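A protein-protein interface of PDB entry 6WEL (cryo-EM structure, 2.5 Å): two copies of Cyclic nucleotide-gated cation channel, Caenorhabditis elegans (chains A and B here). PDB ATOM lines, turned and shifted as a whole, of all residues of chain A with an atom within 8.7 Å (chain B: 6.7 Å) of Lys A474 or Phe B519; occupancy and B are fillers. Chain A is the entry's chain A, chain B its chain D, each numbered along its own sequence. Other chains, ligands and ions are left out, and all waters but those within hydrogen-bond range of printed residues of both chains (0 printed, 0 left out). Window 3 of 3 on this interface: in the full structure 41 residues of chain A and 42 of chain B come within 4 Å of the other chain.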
ATOM      1  N   LEU A 471     -18.886   0.259 -14.500  1.00  0.00           N
ATOM      2  CA  LEU A 471     -19.452   1.224 -13.578  1.00  0.00           C
ATOM      3  C   LEU A 471     -20.581   1.993 -14.235  1.00  0.00           C
ATOM      4  O   LEU A 471     -20.661   2.077 -15.463  1.00  0.00           O
ATOM      5  CB  LEU A 471     -18.378   2.201 -13.100  1.00  0.00           C
ATOM      6  CG  LEU A 471     -17.275   1.648 -12.213  1.00  0.00           C
ATOM      7  CD1 LEU A 471     -16.305   2.741 -11.889  1.00  0.00           C
ATOM      8  CD2 LEU A 471     -17.855   1.072 -10.949  1.00  0.00           C
ATOM      9  N   PRO A 472     -21.493   2.552 -13.452  1.00  0.00           N
ATOM     10  CA  PRO A 472     -22.493   3.455 -14.018  1.00  0.00           C
ATOM     11  C   PRO A 472     -21.883   4.794 -14.405  1.00  0.00           C
ATOM     12  O   PRO A 472     -20.918   5.264 -13.809  1.00  0.00           O
ATOM     13  CB  PRO A 472     -23.512   3.613 -12.885  1.00  0.00           C
ATOM     14  CG  PRO A 472     -22.822   3.168 -11.670  1.00  0.00           C
ATOM     15  CD  PRO A 472     -21.837   2.146 -12.082  1.00  0.00           C
ATOM     16  N   ASP A 473     -22.493   5.410 -15.416  1.00  0.00           N
ATOM     17  CA  ASP A 473     -21.946   6.623 -16.015  1.00  0.00           C
ATOM     18  C   ASP A 473     -21.746   7.739 -15.002  1.00  0.00           C
ATOM     19  O   ASP A 473     -20.890   8.604 -15.201  1.00  0.00           O
ATOM     20  CB  ASP A 473     -22.854   7.098 -17.139  1.00  0.00           C
ATOM     21  CG  ASP A 473     -23.045   6.054 -18.207  1.00  0.00           C
ATOM     22  OD1 ASP A 473     -22.632   4.900 -17.981  1.00  0.00           O
ATOM     23  OD2 ASP A 473     -23.600   6.383 -19.275  1.00  0.00           O
ATOM     24  N   LYS A 474     -22.519   7.748 -13.924  1.00  0.00           N
ATOM     25  CA  LYS A 474     -22.298   8.736 -12.876  1.00  0.00           C
ATOM     26  C   LYS A 474     -20.927   8.556 -12.243  1.00  0.00           C
ATOM     27  O   LYS A 474     -20.161   9.517 -12.110  1.00  0.00           O
ATOM     28  CB  LYS A 474     -23.398   8.621 -11.822  1.00  0.00           C
ATOM     29  CG  LYS A 474     -23.304   9.641 -10.717  1.00  0.00           C
ATOM     30  CD  LYS A 474     -23.700  11.010 -11.203  1.00  0.00           C
ATOM     31  CE  LYS A 474     -23.577  12.026 -10.102  1.00  0.00           C
ATOM     32  NZ  LYS A 474     -23.932  13.372 -10.595  1.00  0.00           N
ATOM     33  N   LEU A 475     -20.591   7.322 -11.866  1.00  0.00           N
ATOM     34  CA  LEU A 475     -19.293   7.064 -11.258  1.00  0.00           C
ATOM     35  C   LEU A 475     -18.163   7.269 -12.250  1.00  0.00           C
ATOM     36  O   LEU A 475     -17.094   7.755 -11.881  1.00  0.00           O
ATOM     37  CB  LEU A 475     -19.246   5.651 -10.697  1.00  0.00           C
ATOM     38  CG  LEU A 475     -19.884   5.429  -9.334  1.00  0.00           C
ATOM     39  CD1 LEU A 475     -19.607   4.020  -8.868  1.00  0.00           C
ATOM     40  CD2 LEU A 475     -19.364   6.434  -8.337  1.00  0.00           C
ATOM     41  N   GLN A 476     -18.374   6.889 -13.512  1.00  0.00           N
ATOM     42  CA  GLN A 476     -17.355   7.109 -14.528  1.00  0.00           C
ATOM     43  C   GLN A 476     -17.066   8.588 -14.698  1.00  0.00           C
ATOM     44  O   GLN A 476     -15.902   8.993 -14.774  1.00  0.00           O
ATOM     45  CB  GLN A 476     -17.795   6.510 -15.856  1.00  0.00           C
ATOM     46  CG  GLN A 476     -17.909   5.020 -15.843  1.00  0.00           C
ATOM     47  CD  GLN A 476     -18.327   4.481 -17.175  1.00  0.00           C
ATOM     48  OE1 GLN A 476     -18.028   5.065 -18.209  1.00  0.00           O
ATOM     49  NE2 GLN A 476     -19.032   3.368 -17.165  1.00  0.00           N
ATOM     50  N   ALA A 477     -18.112   9.409 -14.749  1.00  0.00           N
ATOM     51  CA  ALA A 477     -17.915  10.846 -14.886  1.00  0.00           C
ATOM     52  C   ALA A 477     -17.218  11.426 -13.667  1.00  0.00           C
ATOM     53  O   ALA A 477     -16.345  12.283 -13.804  1.00  0.00           O
ATOM     54  CB  ALA A 477     -19.252  11.537 -15.119  1.00  0.00           C
ATOM     55  N   GLU A 478     -17.583  10.975 -12.468  1.00  0.00           N
ATOM     56  CA  GLU A 478     -16.935  11.501 -11.269  1.00  0.00           C
ATOM     57  C   GLU A 478     -15.465  11.113 -11.210  1.00  0.00           C
ATOM     58  O   GLU A 478     -14.613  11.938 -10.860  1.00  0.00           O
ATOM     59  CB  GLU A 478     -17.651  11.004 -10.022  1.00  0.00           C
ATOM     60  CG  GLU A 478     -19.075  11.449  -9.908  1.00  0.00           C
ATOM     61  CD  GLU A 478     -19.715  10.921  -8.661  1.00  0.00           C
ATOM     62  OE1 GLU A 478     -18.996  10.311  -7.848  1.00  0.00           O
ATOM     63  OE2 GLU A 478     -20.936  11.108  -8.486  1.00  0.00           O
ATOM     64  N   ILE A 479     -15.147   9.864 -11.537  1.00  0.00           N
ATOM     65  CA  ILE A 479     -13.758   9.423 -11.535  1.00  0.00           C
ATOM     66  C   ILE A 479     -12.957  10.184 -12.575  1.00  0.00           C
ATOM     67  O   ILE A 479     -11.826  10.601 -12.319  1.00  0.00           O
ATOM     68  CB  ILE A 479     -13.680   7.903 -11.758  1.00  0.00           C
ATOM     69  CG1 ILE A 479     -14.257   7.166 -10.557  1.00  0.00           C
ATOM     70  CG2 ILE A 479     -12.260   7.471 -12.001  1.00  0.00           C
ATOM     71  CD1 ILE A 479     -14.401   5.693 -10.759  1.00  0.00           C
ATOM     72  N   ALA A 480     -13.529  10.392 -13.761  1.00  0.00           N
ATOM     73  CA  ALA A 480     -12.808  11.112 -14.803  1.00  0.00           C
ATOM     74  C   ALA A 480     -12.617  12.575 -14.439  1.00  0.00           C
ATOM     75  O   ALA A 480     -11.588  13.168 -14.760  1.00  0.00           O
ATOM     76  CB  ALA A 480     -13.543  10.978 -16.131  1.00  0.00           C
ATOM     77  N   MET A 481     -13.601  13.183 -13.782  1.00  0.00           N
ATOM     78  CA  MET A 481     -13.468  14.581 -13.390  1.00  0.00           C
ATOM     79  C   MET A 481     -12.449  14.744 -12.281  1.00  0.00           C
ATOM     80  O   MET A 481     -11.785  15.775 -12.188  1.00  0.00           O
ATOM     81  CB  MET A 481     -14.816  15.143 -12.948  1.00  0.00           C
ATOM     82  CG  MET A 481     -15.770  15.447 -14.076  1.00  0.00           C
ATOM     83  SD  MET A 481     -15.530  17.090 -14.748  1.00  0.00           S
ATOM     84  CE  MET A 481     -15.764  18.062 -13.272  1.00  0.00           C
ATOM     85  N   LEU A 507     -14.159  13.483 -20.343  1.00  0.00           N
ATOM     86  CA  LEU A 507     -14.662  12.166 -20.723  1.00  0.00           C
ATOM     87  C   LEU A 507     -13.903  11.582 -21.911  1.00  0.00           C
ATOM     88  O   LEU A 507     -13.663  10.372 -21.953  1.00  0.00           O
ATOM     89  CB  LEU A 507     -16.155  12.243 -21.021  1.00  0.00           C
ATOM     90  CG  LEU A 507     -16.995  12.135 -19.755  1.00  0.00           C
ATOM     91  CD1 LEU A 507     -18.461  12.215 -20.085  1.00  0.00           C
ATOM     92  CD2 LEU A 507     -16.672  10.843 -19.031  1.00  0.00           C
ATOM     93  N   ARG B 447     -16.774   5.313  -2.045  1.00  0.00           N
ATOM     94  CA  ARG B 447     -18.070   5.467  -2.700  1.00  0.00           C
ATOM     95  C   ARG B 447     -18.236   4.483  -3.857  1.00  0.00           C
ATOM     96  O   ARG B 447     -19.296   3.862  -4.014  1.00  0.00           O
ATOM     97  CB  ARG B 447     -18.221   6.904  -3.175  1.00  0.00           C
ATOM     98  CG  ARG B 447     -19.304   7.130  -4.179  1.00  0.00           C
ATOM     99  CD  ARG B 447     -19.637   8.595  -4.227  1.00  0.00           C
ATOM    100  NE  ARG B 447     -20.333   8.965  -5.449  1.00  0.00           N
ATOM    101  CZ  ARG B 447     -21.630   8.780  -5.648  1.00  0.00           C
ATOM    102  NH1 ARG B 447     -22.370   8.219  -4.707  1.00  0.00           N
ATOM    103  NH2 ARG B 447     -22.179   9.153  -6.791  1.00  0.00           N
ATOM    104  N   TRP B 451     -21.018   1.385  -3.981  1.00  0.00           N
ATOM    105  CA  TRP B 451     -21.993   1.212  -5.050  1.00  0.00           C
ATOM    106  C   TRP B 451     -21.832  -0.142  -5.726  1.00  0.00           C
ATOM    107  O   TRP B 451     -22.824  -0.803  -6.050  1.00  0.00           O
ATOM    108  CB  TRP B 451     -21.858   2.349  -6.055  1.00  0.00           C
ATOM    109  CG  TRP B 451     -23.061   2.578  -6.905  1.00  0.00           C
ATOM    110  CD1 TRP B 451     -24.068   1.702  -7.163  1.00  0.00           C
ATOM    111  CD2 TRP B 451     -23.386   3.779  -7.606  1.00  0.00           C
ATOM    112  NE1 TRP B 451     -24.995   2.278  -7.990  1.00  0.00           N
ATOM    113  CE2 TRP B 451     -24.597   3.556  -8.274  1.00  0.00           C
ATOM    114  CE3 TRP B 451     -22.765   5.019  -7.736  1.00  0.00           C
ATOM    115  CZ2 TRP B 451     -25.192   4.525  -9.064  1.00  0.00           C
ATOM    116  CZ3 TRP B 451     -23.360   5.976  -8.520  1.00  0.00           C
ATOM    117  CH2 TRP B 451     -24.559   5.726  -9.171  1.00  0.00           C
ATOM    118  N   VAL B 513     -28.560   4.171 -13.559  1.00  0.00           N
ATOM    119  CA  VAL B 513     -28.743   3.980 -12.130  1.00  0.00           C
ATOM    120  C   VAL B 513     -28.036   5.102 -11.389  1.00  0.00           C
ATOM    121  O   VAL B 513     -26.996   5.596 -11.832  1.00  0.00           O
ATOM    122  CB  VAL B 513     -28.233   2.601 -11.674  1.00  0.00           C
ATOM    123  CG1 VAL B 513     -28.827   1.533 -12.535  1.00  0.00           C
ATOM    124  CG2 VAL B 513     -26.740   2.539 -11.739  1.00  0.00           C
ATOM    125  N   PHE B 514     -28.619   5.520 -10.272  1.00  0.00           N
ATOM    126  CA  PHE B 514     -28.072   6.573  -9.438  1.00  0.00           C
ATOM    127  C   PHE B 514     -28.081   6.119  -7.987  1.00  0.00           C
ATOM    128  O   PHE B 514     -28.883   5.279  -7.586  1.00  0.00           O
ATOM    129  CB  PHE B 514     -28.866   7.867  -9.596  1.00  0.00           C
ATOM    130  CG  PHE B 514     -28.848   8.411 -10.987  1.00  0.00           C
ATOM    131  CD1 PHE B 514     -29.745   7.961 -11.933  1.00  0.00           C
ATOM    132  CD2 PHE B 514     -27.929   9.368 -11.356  1.00  0.00           C
ATOM    133  CE1 PHE B 514     -29.722   8.453 -13.212  1.00  0.00           C
ATOM    134  CE2 PHE B 514     -27.909   9.859 -12.637  1.00  0.00           C
ATOM    135  CZ  PHE B 514     -28.807   9.402 -13.561  1.00  0.00           C
ATOM    136  N   SER B 515     -27.173   6.667  -7.208  1.00  0.00           N
ATOM    137  CA  SER B 515     -27.023   6.347  -5.801  1.00  0.00           C
ATOM    138  C   SER B 515     -27.664   7.433  -4.959  1.00  0.00           C
ATOM    139  O   SER B 515     -28.106   8.457  -5.482  1.00  0.00           O
ATOM    140  CB  SER B 515     -25.541   6.186  -5.464  1.00  0.00           C
ATOM    141  OG  SER B 515     -24.862   7.417  -5.523  1.00  0.00           O
ATOM    142  N   GLY B 517     -28.513  10.642  -3.109  1.00  0.00           N
ATOM    143  CA  GLY B 517     -27.999  11.991  -3.129  1.00  0.00           C
ATOM    144  C   GLY B 517     -27.399  12.443  -4.438  1.00  0.00           C
ATOM    145  O   GLY B 517     -27.075  13.625  -4.569  1.00  0.00           O
ATOM    146  N   ASP B 518     -27.231  11.548  -5.405  1.00  0.00           N
ATOM    147  CA  ASP B 518     -26.709  11.930  -6.706  1.00  0.00           C
ATOM    148  C   ASP B 518     -27.673  12.860  -7.419  1.00  0.00           C
ATOM    149  O   ASP B 518     -28.891  12.716  -7.310  1.00  0.00           O
ATOM    150  CB  ASP B 518     -26.464  10.696  -7.565  1.00  0.00           C
ATOM    151  CG  ASP B 518     -25.248   9.928  -7.137  1.00  0.00           C
ATOM    152  OD1 ASP B 518     -24.613  10.330  -6.144  1.00  0.00           O
ATOM    153  OD2 ASP B 518     -24.921   8.921  -7.788  1.00  0.00           O
ATOM    154  N   PHE B 519     -27.121  13.812  -8.157  1.00  0.00           N
ATOM    155  CA  PHE B 519     -27.920  14.739  -8.941  1.00  0.00           C
ATOM    156  C   PHE B 519     -28.142  14.169 -10.334  1.00  0.00           C
ATOM    157  O   PHE B 519     -27.185  13.822 -11.027  1.00  0.00           O
ATOM    158  CB  PHE B 519     -27.244  16.103  -9.021  1.00  0.00           C
ATOM    159  CG  PHE B 519     -27.583  17.003  -7.884  1.00  0.00           C
ATOM    160  CD1 PHE B 519     -26.838  16.987  -6.730  1.00  0.00           C
ATOM    161  CD2 PHE B 519     -28.654  17.862  -7.967  1.00  0.00           C
ATOM    162  CE1 PHE B 519     -27.150  17.812  -5.687  1.00  0.00           C
ATOM    163  CE2 PHE B 519     -28.972  18.686  -6.923  1.00  0.00           C
ATOM    164  CZ  PHE B 519     -28.219  18.663  -5.784  1.00  0.00           C
ATOM    165  N   ILE B 520     -29.408  14.064 -10.733  1.00  0.00           N
ATOM    166  CA  ILE B 520     -29.723  13.660 -12.097  1.00  0.00           C
ATOM    167  C   ILE B 520     -29.345  14.766 -13.067  1.00  0.00           C
ATOM    168  O   ILE B 520     -28.793  14.512 -14.143  1.00  0.00           O
ATOM    169  CB  ILE B 520     -31.213  13.296 -12.214  1.00  0.00           C
ATOM    170  CG1 ILE B 520     -31.674  12.473 -11.010  1.00  0.00           C
ATOM    171  CG2 ILE B 520     -31.479  12.565 -13.500  1.00  0.00           C
ATOM    172  CD1 ILE B 520     -30.938  11.202 -10.810  1.00  0.00           C
ATOM    173  N   CYS B 521     -29.630  16.011 -12.695  1.00  0.00           N
ATOM    174  CA  CYS B 521     -29.387  17.173 -13.534  1.00  0.00           C
ATOM    175  C   CYS B 521     -29.333  18.391 -12.632  1.00  0.00           C
ATOM    176  O   CYS B 521     -29.802  18.360 -11.494  1.00  0.00           O
ATOM    177  CB  CYS B 521     -30.476  17.338 -14.599  1.00  0.00           C
ATOM    178  SG  CYS B 521     -32.126  17.632 -13.954  1.00  0.00           S
ATOM    179  N   LYS B 522     -28.750  19.465 -13.148  1.00  0.00           N
ATOM    180  CA  LYS B 522     -28.658  20.711 -12.408  1.00  0.00           C
ATOM    181  C   LYS B 522     -29.049  21.871 -13.307  1.00  0.00           C
ATOM    182  O   LYS B 522     -29.161  21.728 -14.524  1.00  0.00           O
ATOM    183  CB  LYS B 522     -27.255  20.922 -11.835  1.00  0.00           C
ATOM    184  CG  LYS B 522     -27.158  20.564 -10.368  1.00  0.00           C
ATOM    185  CD  LYS B 522     -25.728  20.442  -9.907  1.00  0.00           C
ATOM    186  CE  LYS B 522     -25.660  20.376  -8.395  1.00  0.00           C
ATOM    187  NZ  LYS B 522     -24.276  20.156  -7.904  1.00  0.00           N
ATOM    188  N   GLN B 539     -36.448  13.966  -6.354  1.00  0.00           N
ATOM    189  CA  GLN B 539     -37.049  15.171  -5.800  1.00  0.00           C
ATOM    190  C   GLN B 539     -36.337  16.391  -6.357  1.00  0.00           C
ATOM    191  O   GLN B 539     -35.124  16.370  -6.562  1.00  0.00           O
ATOM    192  CB  GLN B 539     -36.999  15.165  -4.271  1.00  0.00           C
ATOM    193  CG  GLN B 539     -35.623  15.248  -3.683  1.00  0.00           C
ATOM    194  CD  GLN B 539     -35.637  15.068  -2.192  1.00  0.00           C
ATOM    195  OE1 GLN B 539     -36.601  14.553  -1.633  1.00  0.00           O
ATOM    196  NE2 GLN B 539     -34.569  15.493  -1.530  1.00  0.00           N
ATOM    197  N   VAL B 541     -34.985  19.928  -5.951  1.00  0.00           N
ATOM    198  CA  VAL B 541     -34.473  20.694  -4.822  1.00  0.00           C
ATOM    199  C   VAL B 541     -34.114  22.096  -5.290  1.00  0.00           C
ATOM    200  O   VAL B 541     -33.621  22.283  -6.408  1.00  0.00           O
ATOM    201  CB  VAL B 541     -33.269  19.997  -4.183  1.00  0.00           C
ATOM    202  CG1 VAL B 541     -33.715  18.698  -3.577  1.00  0.00           C
ATOM    203  CG2 VAL B 541     -32.197  19.752  -5.220  1.00  0.00           C
ATOM    204  N   ASP B 544     -30.003  24.674  -3.591  1.00  0.00           N
ATOM    205  CA  ASP B 544     -29.053  24.514  -2.501  1.00  0.00           C
ATOM    206  C   ASP B 544     -29.072  23.119  -1.905  1.00  0.00           C
ATOM    207  O   ASP B 544     -28.148  22.758  -1.171  1.00  0.00           O
ATOM    208  CB  ASP B 544     -29.323  25.552  -1.408  1.00  0.00           C
ATOM    209  CG  ASP B 544     -28.197  25.636  -0.401  1.00  0.00           C
ATOM    210  OD1 ASP B 544     -27.024  25.718  -0.827  1.00  0.00           O
ATOM    211  OD2 ASP B 544     -28.482  25.620   0.815  1.00  0.00           O
ATOM    212  N   GLY B 545     -30.085  22.321  -2.208  1.00  0.00           N
ATOM    213  CA  GLY B 545     -30.185  21.030  -1.578  1.00  0.00           C
ATOM    214  C   GLY B 545     -30.785  21.074  -0.199  1.00  0.00           C
ATOM    215  O   GLY B 545     -30.737  20.071   0.519  1.00  0.00           O
ATOM    216  N   ASN B 578     -33.123  21.457 -10.783  1.00  0.00           N
ATOM    217  CA  ASN B 578     -32.236  20.524 -10.096  1.00  0.00           C
ATOM    218  C   ASN B 578     -33.053  19.312  -9.682  1.00  0.00           C
ATOM    219  O   ASN B 578     -34.159  19.459  -9.160  1.00  0.00           O
ATOM    220  CB  ASN B 578     -31.601  21.156  -8.858  1.00  0.00           C
ATOM    221  CG  ASN B 578     -31.013  22.518  -9.124  1.00  0.00           C
ATOM    222  OD1 ASN B 578     -29.797  22.688  -9.128  1.00  0.00           O
ATOM    223  ND2 ASN B 578     -31.872  23.506  -9.316  1.00  0.00           N
ATOM    224  N   VAL B 579     -32.522  18.118  -9.927  1.00  0.00           N
ATOM    225  CA  VAL B 579     -33.199  16.881  -9.556  1.00  0.00           C
ATOM    226  C   VAL B 579     -32.156  15.938  -8.985  1.00  0.00           C
ATOM    227  O   VAL B 579     -31.167  15.629  -9.655  1.00  0.00           O
ATOM    228  CB  VAL B 579     -33.917  16.220 -10.743  1.00  0.00           C
ATOM    229  CG1 VAL B 579     -34.454  14.885 -10.335  1.00  0.00           C
ATOM    230  CG2 VAL B 579     -35.043  17.092 -11.239  1.00  0.00           C
ATOM    231  N   ARG B 580     -32.366  15.483  -7.757  1.00  0.00           N
ATOM    232  CA  ARG B 580     -31.449  14.557  -7.124  1.00  0.00           C
ATOM    233  C   ARG B 580     -32.189  13.315  -6.656  1.00  0.00           C
ATOM    234  O   ARG B 580     -33.389  13.349  -6.383  1.00  0.00           O
ATOM    235  CB  ARG B 580     -30.717  15.198  -5.951  1.00  0.00           C
ATOM    236  CG  ARG B 580     -31.588  15.625  -4.822  1.00  0.00           C
ATOM    237  CD  ARG B 580     -30.834  15.524  -3.520  1.00  0.00           C
ATOM    238  NE  ARG B 580     -31.637  15.992  -2.400  1.00  0.00           N
ATOM    239  CZ  ARG B 580     -31.387  17.104  -1.722  1.00  0.00           C
ATOM    240  NH1 ARG B 580     -32.174  17.460  -0.722  1.00  0.00           N
ATOM    241  NH2 ARG B 580     -30.345  17.851  -2.043  1.00  0.00           N
ATOM    242  N   SER B 581     -31.448  12.216  -6.581  1.00  0.00           N
ATOM    243  CA  SER B 581     -31.995  10.930  -6.192  1.00  0.00           C
ATOM    244  C   SER B 581     -32.052  10.809  -4.678  1.00  0.00           C
ATOM    245  O   SER B 581     -31.111  11.188  -3.977  1.00  0.00           O
ATOM    246  CB  SER B 581     -31.138   9.813  -6.776  1.00  0.00           C
ATOM    247  OG  SER B 581     -31.561   8.549  -6.322  1.00  0.00           O
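OE2 of Glu A478 lies within salt-bridge range of NH2 of Arg B447 (2.9 Å).
The side-chain amino group of Lys A474 sits at hydrogen-bond distance from the backbone carbonyl oxygen of Phe B519 (3.3 Å).
The backbone carbonyl oxygen of Asp B518 is in hydrogen-bond range of the backbone NH of Ser B581 (2.7 Å).
OD2 of Asp B518 sits at hydrogen-bond distance from OG of Ser B515.
The guanidinium group (NH2) of Arg B447 lies within salt-bridge range of the side-chain carboxylate (OD1) of Asp B518.
OG of Ser B515 sits at hydrogen-bond distance from NH1 of Arg B447, at 2.7 Å.
Among the printed residues, pairs that only touch across the chains: Leu A475 with Trp B451 (3.3 Å), Lys A474 with Asp B518 (3.4 Å), Pro A472 with Val B513 (3.6 Å), Pro A472 with Trp B451 (3.8 Å) and Leu A475 with Arg B447 (3.96 Å).
Of the printed residues of chain B, Lys A474 touches Asp B518 (3.4 Å) and Phe B519 (3.3 Å).
Phe B519 touches just one residue of chain A: Lys A474 (3.3 Å).
Of chain A, only Lys A474 comes within 4 Å of Asp B518.
Of the printed residues of chain A, Trp B451 touches Pro A472 and Leu A475.
Printed residues of chain B within 4 Å of Leu A475: Arg B447 and Trp B451.
Of the printed residues of chain A, Arg B447 touches Leu A475 and Glu A478.
Ile A479 touches none of the printed residues of chain B.
Ser B581 touches none of the printed residues of chain A.
The nearest printed residue of chain B that does not touch Glu A478 is Asp B518 (4.4 Å).
Printed residues of chain A that touch a printed residue of chain B: Pro A472, Lys A474, Leu A475 and Glu A478.
Hydrophobic or aromatic side chains of chain A within 4 Å of the printed part of chain B: Pro A472 and Leu A475.
No position is printed for both chains.
Of the 7 pairs that touch across the chains among the printed residues, none has its exchanged pair printed and touching as well.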
